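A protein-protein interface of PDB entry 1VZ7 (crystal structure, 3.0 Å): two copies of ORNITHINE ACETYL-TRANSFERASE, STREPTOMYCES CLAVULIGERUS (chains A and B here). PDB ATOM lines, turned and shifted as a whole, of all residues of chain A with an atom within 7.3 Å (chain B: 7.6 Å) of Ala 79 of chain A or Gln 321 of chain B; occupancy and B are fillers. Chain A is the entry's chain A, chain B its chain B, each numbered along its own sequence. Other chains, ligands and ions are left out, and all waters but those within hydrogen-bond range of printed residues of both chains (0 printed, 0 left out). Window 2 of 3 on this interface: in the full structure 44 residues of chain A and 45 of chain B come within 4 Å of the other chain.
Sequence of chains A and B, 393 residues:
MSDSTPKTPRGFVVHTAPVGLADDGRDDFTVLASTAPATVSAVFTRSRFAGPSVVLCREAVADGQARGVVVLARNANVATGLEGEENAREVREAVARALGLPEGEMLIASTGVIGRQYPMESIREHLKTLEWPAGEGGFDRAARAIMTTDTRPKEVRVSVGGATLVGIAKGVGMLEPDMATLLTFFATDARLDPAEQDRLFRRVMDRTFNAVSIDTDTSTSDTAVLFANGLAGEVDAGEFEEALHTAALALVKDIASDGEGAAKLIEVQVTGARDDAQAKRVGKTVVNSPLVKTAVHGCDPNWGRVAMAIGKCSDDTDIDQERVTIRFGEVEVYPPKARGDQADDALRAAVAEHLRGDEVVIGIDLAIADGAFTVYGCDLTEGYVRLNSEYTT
The guanidinium group (NH1) of Arg 48 of chain A sits close to the backbone carbonyl oxygen (O) of Ile 319 of chain B, at 3.3 Å. NH1 of Arg 48 of chain A sits at hydrogen-bond distance from O of Thr 317 of chain B (2.6 Å).
O of Val 78 of chain A sits at hydrogen-bond distance from N of Gly 115 of chain A (3.2 Å). OG of Ser 47 of chain A lies close to N of Phe 49 of chain A. The backbone carbonyl oxygen (O) of Gln 321 of chain B lies within hydrogen-bond range of the side-chain hydroxyl (OH) of Tyr 334 of chain B, at 3.1 Å.
Among the printed residues, merely in contact across the chains: Arg 48 of chain A with Gln 321 of chain B (3.5 Å), Phe 49 of chain A with Ala 307 of chain B (3.3 Å), Phe 49 of chain A with Gln 321 of chain B (3.5 Å), Phe 49 of chain A with Tyr 334 of chain B (3.7 Å), Ala 50 of chain A with Gln 321 of chain B (3.8 Å), Ala 79 of chain A with Trp 303 of chain B (3.4 Å), Ala 79 of chain A with Gln 321 of chain B (3.9 Å), Ile 114 of chain A with Gly 304 of chain B (3.7 Å) and Gly 115 of chain A with Trp 303 of chain B (3.5 Å).
Printed residues of chain B within 4 Å of Arg 48 of chain A: Thr 317 (2.6 Å), Ile 319 (3.3 Å) and Gln 321 (3.5 Å). Printed residues of chain B within 4 Å of Ala 50 of chain A: Gln 321 (3.8 Å). Of chain B, only Trp 303 and Gln 321 come within 4 Å of Ala 79 of chain A. Gly 84 of chain A touches none of the printed residues of chain B. Of the printed residues of chain B, Ile 114 of chain A touches Gly 304. Printed residues of chain A within 4 Å of Gly 304 of chain B: Ile 114. Of chain A, only Arg 48 (3.5 Å), Phe 49 (3.5 Å), Ala 50 (3.8 Å) and Ala 79 (3.9 Å) come within 4 Å of Gln 321 of chain B. Leu 366 of chain B touches none of the printed residues of chain A. The nearest residue of chain A that does not touch Gln 321 of chain B is Val 78 of chain A (4.9 Å). The nearest printed residue of chain B that does not touch Gly 115 of chain A is Pro 336 of chain B (5.3 Å).
Hydrophobic or aromatic side chains of chain B that line the printed part of chain A: Trp 303, Ala 307, Ile 319 and Tyr 334.
No position is printed for both chains. Of the 11 pairs that touch across the chains among the printed residues, none has its exchanged pair printed and touching as well.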
ATOM      1  N   SER A  47       9.590 -15.538   1.940  1.00  0.00           N
ATOM      2  CA  SER A  47       8.659 -16.525   2.481  1.00  0.00           C
ATOM      3  C   SER A  47       7.422 -16.535   1.609  1.00  0.00           C
ATOM      4  O   SER A  47       7.099 -15.514   1.007  1.00  0.00           O
ATOM      5  CB  SER A  47       8.265 -16.149   3.918  1.00  0.00           C
ATOM      6  OG  SER A  47       7.367 -17.091   4.483  1.00  0.00           O
ATOM      7  N   ARG A  48       6.738 -17.672   1.516  1.00  0.00           N
ATOM      8  CA  ARG A  48       5.512 -17.739   0.715  1.00  0.00           C
ATOM      9  C   ARG A  48       4.349 -17.213   1.556  1.00  0.00           C
ATOM     10  O   ARG A  48       3.257 -16.941   1.053  1.00  0.00           O
ATOM     11  CB  ARG A  48       5.237 -19.176   0.284  1.00  0.00           C
ATOM     12  CG  ARG A  48       6.003 -19.617  -0.961  1.00  0.00           C
ATOM     13  CD  ARG A  48       5.336 -19.159  -2.236  1.00  0.00           C
ATOM     14  NE  ARG A  48       5.593 -17.755  -2.516  1.00  0.00           N
ATOM     15  CZ  ARG A  48       5.084 -17.081  -3.549  1.00  0.00           C
ATOM     16  NH1 ARG A  48       4.281 -17.676  -4.410  1.00  0.00           N
ATOM     17  NH2 ARG A  48       5.376 -15.806  -3.713  1.00  0.00           N
ATOM     18  N   PHE A  49       4.619 -17.076   2.849  1.00  0.00           N
ATOM     19  CA  PHE A  49       3.664 -16.573   3.817  1.00  0.00           C
ATOM     20  C   PHE A  49       4.155 -15.229   4.342  1.00  0.00           C
ATOM     21  O   PHE A  49       4.013 -14.915   5.526  1.00  0.00           O
ATOM     22  CB  PHE A  49       3.528 -17.544   4.987  1.00  0.00           C
ATOM     23  CG  PHE A  49       2.346 -18.449   4.889  1.00  0.00           C
ATOM     24  CD1 PHE A  49       2.399 -19.606   4.133  1.00  0.00           C
ATOM     25  CD2 PHE A  49       1.170 -18.139   5.559  1.00  0.00           C
ATOM     26  CE1 PHE A  49       1.302 -20.442   4.047  1.00  0.00           C
ATOM     27  CE2 PHE A  49       0.061 -18.970   5.480  1.00  0.00           C
ATOM     28  CZ  PHE A  49       0.125 -20.123   4.724  1.00  0.00           C
ATOM     29  N   ALA A  50       4.749 -14.439   3.460  1.00  0.00           N
ATOM     30  CA  ALA A  50       5.251 -13.129   3.840  1.00  0.00           C
ATOM     31  C   ALA A  50       4.112 -12.213   4.321  1.00  0.00           C
ATOM     32  O   ALA A  50       3.141 -11.966   3.601  1.00  0.00           O
ATOM     33  CB  ALA A  50       5.974 -12.511   2.660  1.00  0.00           C
ATOM     34  N   GLY A  51       4.234 -11.717   5.546  1.00  0.00           N
ATOM     35  CA  GLY A  51       3.205 -10.848   6.100  1.00  0.00           C
ATOM     36  C   GLY A  51       2.965  -9.602   5.277  1.00  0.00           C
ATOM     37  O   GLY A  51       3.889  -9.111   4.642  1.00  0.00           O
ATOM     38  N   PRO A  52       1.744  -9.044   5.291  1.00  0.00           N
ATOM     39  CA  PRO A  52       1.460  -7.841   4.504  1.00  0.00           C
ATOM     40  C   PRO A  52       2.476  -6.717   4.734  1.00  0.00           C
ATOM     41  O   PRO A  52       2.660  -5.853   3.872  1.00  0.00           O
ATOM     42  CB  PRO A  52       0.035  -7.480   4.936  1.00  0.00           C
ATOM     43  CG  PRO A  52       0.013  -7.898   6.346  1.00  0.00           C
ATOM     44  CD  PRO A  52       0.682  -9.259   6.289  1.00  0.00           C
ATOM     45  N   VAL A  55       5.169  -6.963   2.107  1.00  0.00           N
ATOM     46  CA  VAL A  55       4.790  -6.465   0.780  1.00  0.00           C
ATOM     47  C   VAL A  55       4.928  -4.963   0.693  1.00  0.00           C
ATOM     48  O   VAL A  55       5.501  -4.449  -0.257  1.00  0.00           O
ATOM     49  CB  VAL A  55       3.323  -6.821   0.390  1.00  0.00           C
ATOM     50  CG1 VAL A  55       3.038  -6.355  -1.038  1.00  0.00           C
ATOM     51  CG2 VAL A  55       3.084  -8.316   0.500  1.00  0.00           C
ATOM     52  N   ALA A  76       3.385 -10.520  14.638  1.00  0.00           N
ATOM     53  CA  ALA A  76       3.898 -10.369  13.283  1.00  0.00           C
ATOM     54  C   ALA A  76       2.886  -9.832  12.271  1.00  0.00           C
ATOM     55  O   ALA A  76       3.274  -9.346  11.208  1.00  0.00           O
ATOM     56  CB  ALA A  76       4.429 -11.713  12.798  1.00  0.00           C
ATOM     57  N   ASN A  77       1.599  -9.913  12.609  1.00  0.00           N
ATOM     58  CA  ASN A  77       0.523  -9.503  11.707  1.00  0.00           C
ATOM     59  C   ASN A  77       0.748 -10.228  10.382  1.00  0.00           C
ATOM     60  O   ASN A  77       1.006  -9.622   9.335  1.00  0.00           O
ATOM     61  CB  ASN A  77       0.481  -7.984  11.496  1.00  0.00           C
ATOM     62  CG  ASN A  77      -0.639  -7.558  10.548  1.00  0.00           C
ATOM     63  OD1 ASN A  77      -1.731  -8.128  10.550  1.00  0.00           O
ATOM     64  ND2 ASN A  77      -0.373  -6.542   9.744  1.00  0.00           N
ATOM     65  N   VAL A  78       0.647 -11.549  10.468  1.00  0.00           N
ATOM     66  CA  VAL A  78       0.843 -12.452   9.348  1.00  0.00           C
ATOM     67  C   VAL A  78      -0.321 -13.425   9.409  1.00  0.00           C
ATOM     68  O   VAL A  78      -0.851 -13.672  10.482  1.00  0.00           O
ATOM     69  CB  VAL A  78       2.207 -13.229   9.519  1.00  0.00           C
ATOM     70  CG1 VAL A  78       2.213 -14.535   8.702  1.00  0.00           C
ATOM     71  CG2 VAL A  78       3.380 -12.332   9.095  1.00  0.00           C
ATOM     72  N   ALA A  79      -0.737 -13.967   8.273  1.00  0.00           N
ATOM     73  CA  ALA A  79      -1.824 -14.935   8.298  1.00  0.00           C
ATOM     74  C   ALA A  79      -3.075 -14.342   8.929  1.00  0.00           C
ATOM     75  O   ALA A  79      -3.926 -15.065   9.449  1.00  0.00           O
ATOM     76  CB  ALA A  79      -1.392 -16.171   9.088  1.00  0.00           C
ATOM     77  N   THR A  80      -3.174 -13.023   8.905  1.00  0.00           N
ATOM     78  CA  THR A  80      -4.322 -12.341   9.470  1.00  0.00           C
ATOM     79  C   THR A  80      -5.268 -11.972   8.327  1.00  0.00           C
ATOM     80  O   THR A  80      -6.365 -11.452   8.546  1.00  0.00           O
ATOM     81  CB  THR A  80      -3.875 -11.082  10.237  1.00  0.00           C
ATOM     82  OG1 THR A  80      -2.932 -10.342   9.447  1.00  0.00           O
ATOM     83  CG2 THR A  80      -3.240 -11.471  11.571  1.00  0.00           C
ATOM     84  N   GLY A  81      -4.824 -12.264   7.105  1.00  0.00           N
ATOM     85  CA  GLY A  81      -5.610 -11.992   5.914  1.00  0.00           C
ATOM     86  C   GLY A  81      -5.943 -10.533   5.680  1.00  0.00           C
ATOM     87  O   GLY A  81      -5.172  -9.642   6.036  1.00  0.00           O
ATOM     88  N   LEU A  82      -7.103 -10.301   5.070  1.00  0.00           N
ATOM     89  CA  LEU A  82      -7.589  -8.956   4.760  1.00  0.00           C
ATOM     90  C   LEU A  82      -7.615  -8.076   5.992  1.00  0.00           C
ATOM     91  O   LEU A  82      -6.959  -7.042   6.019  1.00  0.00           O
ATOM     92  CB  LEU A  82      -8.994  -9.014   4.143  1.00  0.00           C
ATOM     93  CG  LEU A  82      -9.706  -7.671   3.938  1.00  0.00           C
ATOM     94  CD1 LEU A  82     -10.480  -7.696   2.634  1.00  0.00           C
ATOM     95  CD2 LEU A  82     -10.627  -7.381   5.120  1.00  0.00           C
ATOM     96  N   GLY A  84      -6.035  -8.175   8.419  1.00  0.00           N
ATOM     97  CA  GLY A  84      -4.616  -7.923   8.593  1.00  0.00           C
ATOM     98  C   GLY A  84      -4.034  -6.881   7.649  1.00  0.00           C
ATOM     99  O   GLY A  84      -3.439  -5.903   8.102  1.00  0.00           O
ATOM    100  N   ILE A 114       2.036 -15.239  15.106  1.00  0.00           N
ATOM    101  CA  ILE A 114       1.372 -15.404  13.825  1.00  0.00           C
ATOM    102  C   ILE A 114      -0.082 -15.820  14.025  1.00  0.00           C
ATOM    103  O   ILE A 114      -0.379 -16.658  14.870  1.00  0.00           O
ATOM    104  CB  ILE A 114       2.076 -16.484  12.988  1.00  0.00           C
ATOM    105  CG1 ILE A 114       3.431 -15.961  12.499  1.00  0.00           C
ATOM    106  CG2 ILE A 114       1.185 -16.913  11.834  1.00  0.00           C
ATOM    107  CD1 ILE A 114       4.369 -17.048  11.983  1.00  0.00           C
ATOM    108  N   GLY A 115      -0.985 -15.216  13.261  1.00  0.00           N
ATOM    109  CA  GLY A 115      -2.383 -15.584  13.359  1.00  0.00           C
ATOM    110  C   GLY A 115      -3.304 -14.678  14.150  1.00  0.00           C
ATOM    111  O   GLY A 115      -4.526 -14.726  13.976  1.00  0.00           O
ATOM    112  N   ARG A 116      -2.738 -13.864  15.029  1.00  0.00           N
ATOM    113  CA  ARG A 116      -3.552 -12.964  15.828  1.00  0.00           C
ATOM    114  C   ARG A 116      -3.506 -11.595  15.192  1.00  0.00           C
ATOM    115  O   ARG A 116      -2.502 -11.231  14.583  1.00  0.00           O
ATOM    116  CB  ARG A 116      -3.034 -12.893  17.265  1.00  0.00           C
ATOM    117  N   GLN A 117      -4.606 -10.855  15.327  1.00  0.00           N
ATOM    118  CA  GLN A 117      -4.735  -9.513  14.772  1.00  0.00           C
ATOM    119  C   GLN A 117      -4.184  -8.468  15.730  1.00  0.00           C
ATOM    120  O   GLN A 117      -4.099  -8.696  16.939  1.00  0.00           O
ATOM    121  CB  GLN A 117      -6.200  -9.195  14.484  1.00  0.00           C
ATOM    122  CG  GLN A 117      -6.858 -10.094  13.454  1.00  0.00           C
ATOM    123  CD  GLN A 117      -6.554  -9.692  12.021  1.00  0.00           C
ATOM    124  OE1 GLN A 117      -5.952  -8.644  11.764  1.00  0.00           O
ATOM    125  NE2 GLN A 117      -6.986 -10.522  11.072  1.00  0.00           N
ATOM    126  N   THR A 220       8.556 -15.516   8.433  1.00  0.00           N
ATOM    127  CA  THR A 220       7.594 -14.934   7.516  1.00  0.00           C
ATOM    128  C   THR A 220       7.720 -13.407   7.614  1.00  0.00           C
ATOM    129  O   THR A 220       6.913 -12.670   7.036  1.00  0.00           O
ATOM    130  CB  THR A 220       6.158 -15.300   7.953  1.00  0.00           C
ATOM    131  OG1 THR A 220       5.937 -14.815   9.288  1.00  0.00           O
ATOM    132  CG2 THR A 220       5.943 -16.806   7.937  1.00  0.00           C
ATOM    133  N   TRP B 303      -0.704 -23.813  14.101  1.00  0.00           N
ATOM    134  CA  TRP B 303      -0.826 -23.810  12.653  1.00  0.00           C
ATOM    135  C   TRP B 303       0.071 -22.727  12.034  1.00  0.00           C
ATOM    136  O   TRP B 303       0.472 -22.824  10.870  1.00  0.00           O
ATOM    137  CB  TRP B 303      -2.287 -23.601  12.226  1.00  0.00           C
ATOM    138  CG  TRP B 303      -2.903 -22.308  12.642  1.00  0.00           C
ATOM    139  CD1 TRP B 303      -3.743 -22.100  13.697  1.00  0.00           C
ATOM    140  CD2 TRP B 303      -2.756 -21.039  11.988  1.00  0.00           C
ATOM    141  NE1 TRP B 303      -4.135 -20.779  13.739  1.00  0.00           N
ATOM    142  CE2 TRP B 303      -3.546 -20.107  12.702  1.00  0.00           C
ATOM    143  CE3 TRP B 303      -2.036 -20.601  10.869  1.00  0.00           C
ATOM    144  CZ2 TRP B 303      -3.640 -18.771  12.335  1.00  0.00           C
ATOM    145  CZ3 TRP B 303      -2.131 -19.270  10.504  1.00  0.00           C
ATOM    146  CH2 TRP B 303      -2.931 -18.368  11.237  1.00  0.00           C
ATOM    147  N   GLY B 304       0.395 -21.708  12.834  1.00  0.00           N
ATOM    148  CA  GLY B 304       1.234 -20.613  12.380  1.00  0.00           C
ATOM    149  C   GLY B 304       2.621 -21.074  12.013  1.00  0.00           C
ATOM    150  O   GLY B 304       3.148 -20.685  10.982  1.00  0.00           O
ATOM    151  N   ALA B 307       2.516 -22.989   8.804  1.00  0.00           N
ATOM    152  CA  ALA B 307       2.448 -22.072   7.668  1.00  0.00           C
ATOM    153  C   ALA B 307       3.830 -21.468   7.419  1.00  0.00           C
ATOM    154  O   ALA B 307       4.273 -21.344   6.269  1.00  0.00           O
ATOM    155  CB  ALA B 307       1.428 -20.968   7.930  1.00  0.00           C
ATOM    156  N   THR B 317       6.680 -20.664  -6.377  1.00  0.00           N
ATOM    157  CA  THR B 317       5.807 -19.502  -6.456  1.00  0.00           C
ATOM    158  C   THR B 317       4.326 -19.771  -6.718  1.00  0.00           C
ATOM    159  O   THR B 317       3.499 -18.877  -6.574  1.00  0.00           O
ATOM    160  CB  THR B 317       6.310 -18.535  -7.523  1.00  0.00           C
ATOM    161  OG1 THR B 317       6.324 -19.198  -8.791  1.00  0.00           O
ATOM    162  CG2 THR B 317       7.717 -18.059  -7.185  1.00  0.00           C
ATOM    163  N   ASP B 318       3.976 -20.986  -7.107  1.00  0.00           N
ATOM    164  CA  ASP B 318       2.579 -21.282  -7.366  1.00  0.00           C
ATOM    165  C   ASP B 318       1.820 -21.565  -6.060  1.00  0.00           C
ATOM    166  O   ASP B 318       0.641 -21.929  -6.074  1.00  0.00           O
ATOM    167  CB  ASP B 318       2.472 -22.454  -8.352  1.00  0.00           C
ATOM    168  CG  ASP B 318       3.133 -23.725  -7.845  1.00  0.00           C
ATOM    169  OD1 ASP B 318       4.124 -23.653  -7.089  1.00  0.00           O
ATOM    170  OD2 ASP B 318       2.662 -24.813  -8.225  1.00  0.00           O
ATOM    171  N   ILE B 319       2.494 -21.383  -4.927  1.00  0.00           N
ATOM    172  CA  ILE B 319       1.863 -21.605  -3.630  1.00  0.00           C
ATOM    173  C   ILE B 319       1.292 -20.302  -3.103  1.00  0.00           C
ATOM    174  O   ILE B 319       2.037 -19.425  -2.656  1.00  0.00           O
ATOM    175  CB  ILE B 319       2.857 -22.140  -2.587  1.00  0.00           C
ATOM    176  CG1 ILE B 319       3.326 -23.535  -2.998  1.00  0.00           C
ATOM    177  CG2 ILE B 319       2.210 -22.152  -1.207  1.00  0.00           C
ATOM    178  CD1 ILE B 319       4.266 -24.200  -2.010  1.00  0.00           C
ATOM    179  N   ASP B 320      -0.031 -20.182  -3.158  1.00  0.00           N
ATOM    180  CA  ASP B 320      -0.696 -18.982  -2.679  1.00  0.00           C
ATOM    181  C   ASP B 320      -1.070 -19.150  -1.219  1.00  0.00           C
ATOM    182  O   ASP B 320      -1.696 -20.134  -0.819  1.00  0.00           O
ATOM    183  CB  ASP B 320      -1.957 -18.700  -3.488  1.00  0.00           C
ATOM    184  CG  ASP B 320      -2.464 -17.288  -3.293  1.00  0.00           C
ATOM    185  OD1 ASP B 320      -2.487 -16.818  -2.134  1.00  0.00           O
ATOM    186  OD2 ASP B 320      -2.843 -16.652  -4.300  1.00  0.00           O
ATOM    187  N   GLN B 321      -0.669 -18.174  -0.426  1.00  0.00           N
ATOM    188  CA  GLN B 321      -0.941 -18.166   0.995  1.00  0.00           C
ATOM    189  C   GLN B 321      -2.454 -18.115   1.254  1.00  0.00           C
ATOM    190  O   GLN B 321      -2.944 -18.644   2.253  1.00  0.00           O
ATOM    191  CB  GLN B 321      -0.233 -16.952   1.600  1.00  0.00           C
ATOM    192  CG  GLN B 321      -0.673 -16.546   2.989  1.00  0.00           C
ATOM    193  CD  GLN B 321      -0.017 -15.262   3.409  1.00  0.00           C
ATOM    194  OE1 GLN B 321      -0.264 -14.743   4.495  1.00  0.00           O
ATOM    195  NE2 GLN B 321       0.832 -14.734   2.542  1.00  0.00           N
ATOM    196  N   GLU B 322      -3.192 -17.487   0.342  1.00  0.00           N
ATOM    197  CA  GLU B 322      -4.639 -17.352   0.478  1.00  0.00           C
ATOM    198  C   GLU B 322      -5.424 -18.614   0.127  1.00  0.00           C
ATOM    199  O   GLU B 322      -6.638 -18.673   0.340  1.00  0.00           O
ATOM    200  CB  GLU B 322      -5.136 -16.199  -0.394  1.00  0.00           C
ATOM    201  CG  GLU B 322      -4.842 -14.823   0.160  1.00  0.00           C
ATOM    202  CD  GLU B 322      -5.287 -13.716  -0.779  1.00  0.00           C
ATOM    203  OE1 GLU B 322      -5.469 -12.573  -0.304  1.00  0.00           O
ATOM    204  OE2 GLU B 322      -5.446 -13.982  -1.989  1.00  0.00           O
ATOM    205  N   ARG B 323      -4.728 -19.618  -0.399  1.00  0.00           N
ATOM    206  CA  ARG B 323      -5.369 -20.870  -0.795  1.00  0.00           C
ATOM    207  C   ARG B 323      -4.985 -22.018   0.126  1.00  0.00           C
ATOM    208  O   ARG B 323      -5.752 -22.954   0.329  1.00  0.00           O
ATOM    209  CB  ARG B 323      -4.978 -21.226  -2.235  1.00  0.00           C
ATOM    210  CG  ARG B 323      -5.092 -20.067  -3.223  1.00  0.00           C
ATOM    211  CD  ARG B 323      -4.592 -20.453  -4.607  1.00  0.00           C
ATOM    212  NE  ARG B 323      -5.521 -21.339  -5.304  1.00  0.00           N
ATOM    213  CZ  ARG B 323      -6.672 -20.943  -5.837  1.00  0.00           C
ATOM    214  NH1 ARG B 323      -7.036 -19.668  -5.752  1.00  0.00           N
ATOM    215  NH2 ARG B 323      -7.460 -21.824  -6.451  1.00  0.00           N
ATOM    216  N   VAL B 324      -3.785 -21.941   0.676  1.00  0.00           N
ATOM    217  CA  VAL B 324      -3.281 -22.973   1.567  1.00  0.00           C
ATOM    218  C   VAL B 324      -4.238 -23.304   2.711  1.00  0.00           C
ATOM    219  O   VAL B 324      -4.700 -22.411   3.423  1.00  0.00           O
ATOM    220  CB  VAL B 324      -1.930 -22.545   2.165  1.00  0.00           C
ATOM    221  CG1 VAL B 324      -1.454 -23.552   3.166  1.00  0.00           C
ATOM    222  CG2 VAL B 324      -0.922 -22.398   1.073  1.00  0.00           C
ATOM    223  N   THR B 325      -4.547 -24.588   2.876  1.00  0.00           N
ATOM    224  CA  THR B 325      -5.412 -25.033   3.966  1.00  0.00           C
ATOM    225  C   THR B 325      -4.650 -26.010   4.838  1.00  0.00           C
ATOM    226  O   THR B 325      -4.089 -26.986   4.345  1.00  0.00           O
ATOM    227  CB  THR B 325      -6.682 -25.741   3.472  1.00  0.00           C
ATOM    228  OG1 THR B 325      -6.374 -26.530   2.318  1.00  0.00           O
ATOM    229  CG2 THR B 325      -7.756 -24.733   3.155  1.00  0.00           C
ATOM    230  N   TYR B 334      -6.902 -23.800   9.474  1.00  0.00           N
ATOM    231  CA  TYR B 334      -6.473 -22.645   8.679  1.00  0.00           C
ATOM    232  C   TYR B 334      -7.010 -22.793   7.259  1.00  0.00           C
ATOM    233  O   TYR B 334      -6.820 -23.833   6.624  1.00  0.00           O
ATOM    234  CB  TYR B 334      -4.947 -22.515   8.595  1.00  0.00           C
ATOM    235  CG  TYR B 334      -4.523 -21.360   7.707  1.00  0.00           C
ATOM    236  CD1 TYR B 334      -4.329 -20.081   8.231  1.00  0.00           C
ATOM    237  CD2 TYR B 334      -4.375 -21.530   6.334  1.00  0.00           C
ATOM    238  CE1 TYR B 334      -3.999 -19.009   7.421  1.00  0.00           C
ATOM    239  CE2 TYR B 334      -4.048 -20.460   5.515  1.00  0.00           C
ATOM    240  CZ  TYR B 334      -3.860 -19.206   6.070  1.00  0.00           C
ATOM    241  OH  TYR B 334      -3.510 -18.149   5.263  1.00  0.00           O
ATOM    242  N   PRO B 335      -7.665 -21.740   6.730  1.00  0.00           N
ATOM    243  CA  PRO B 335      -7.947 -20.426   7.332  1.00  0.00           C
ATOM    244  C   PRO B 335      -8.649 -20.494   8.680  1.00  0.00           C
ATOM    245  O   PRO B 335      -9.467 -21.378   8.910  1.00  0.00           O
ATOM    246  CB  PRO B 335      -8.813 -19.751   6.277  1.00  0.00           C
ATOM    247  CG  PRO B 335      -8.282 -20.307   5.006  1.00  0.00           C
ATOM    248  CD  PRO B 335      -8.150 -21.781   5.342  1.00  0.00           C
ATOM    249  N   PRO B 336      -8.348 -19.552   9.589  1.00  0.00           N
ATOM    250  CA  PRO B 336      -8.991 -19.567  10.910  1.00  0.00           C
ATOM    251  C   PRO B 336     -10.508 -19.417  10.779  1.00  0.00           C
ATOM    252  O   PRO B 336     -11.000 -18.789   9.833  1.00  0.00           O
ATOM    253  CB  PRO B 336      -8.358 -18.369  11.625  1.00  0.00           C
ATOM    254  CG  PRO B 336      -7.087 -18.132  10.880  1.00  0.00           C
ATOM    255  CD  PRO B 336      -7.466 -18.383   9.455  1.00  0.00           C
ATOM    256  N   LEU B 366      -2.100 -27.404  -0.937  1.00  0.00           N
ATOM    257  CA  LEU B 366      -1.579 -26.289  -1.701  1.00  0.00           C
ATOM    258  C   LEU B 366      -2.555 -25.718  -2.738  1.00  0.00           C
ATOM    259  O   LEU B 366      -2.339 -24.632  -3.279  1.00  0.00           O
ATOM    260  CB  LEU B 366      -0.259 -26.717  -2.354  1.00  0.00           C
ATOM    261  CG  LEU B 366       0.764 -27.320  -1.377  1.00  0.00           C
ATOM    262  CD1 LEU B 366       2.132 -27.315  -2.030  1.00  0.00           C
ATOM    263  CD2 LEU B 366       0.811 -26.523  -0.085  1.00  0.00           C
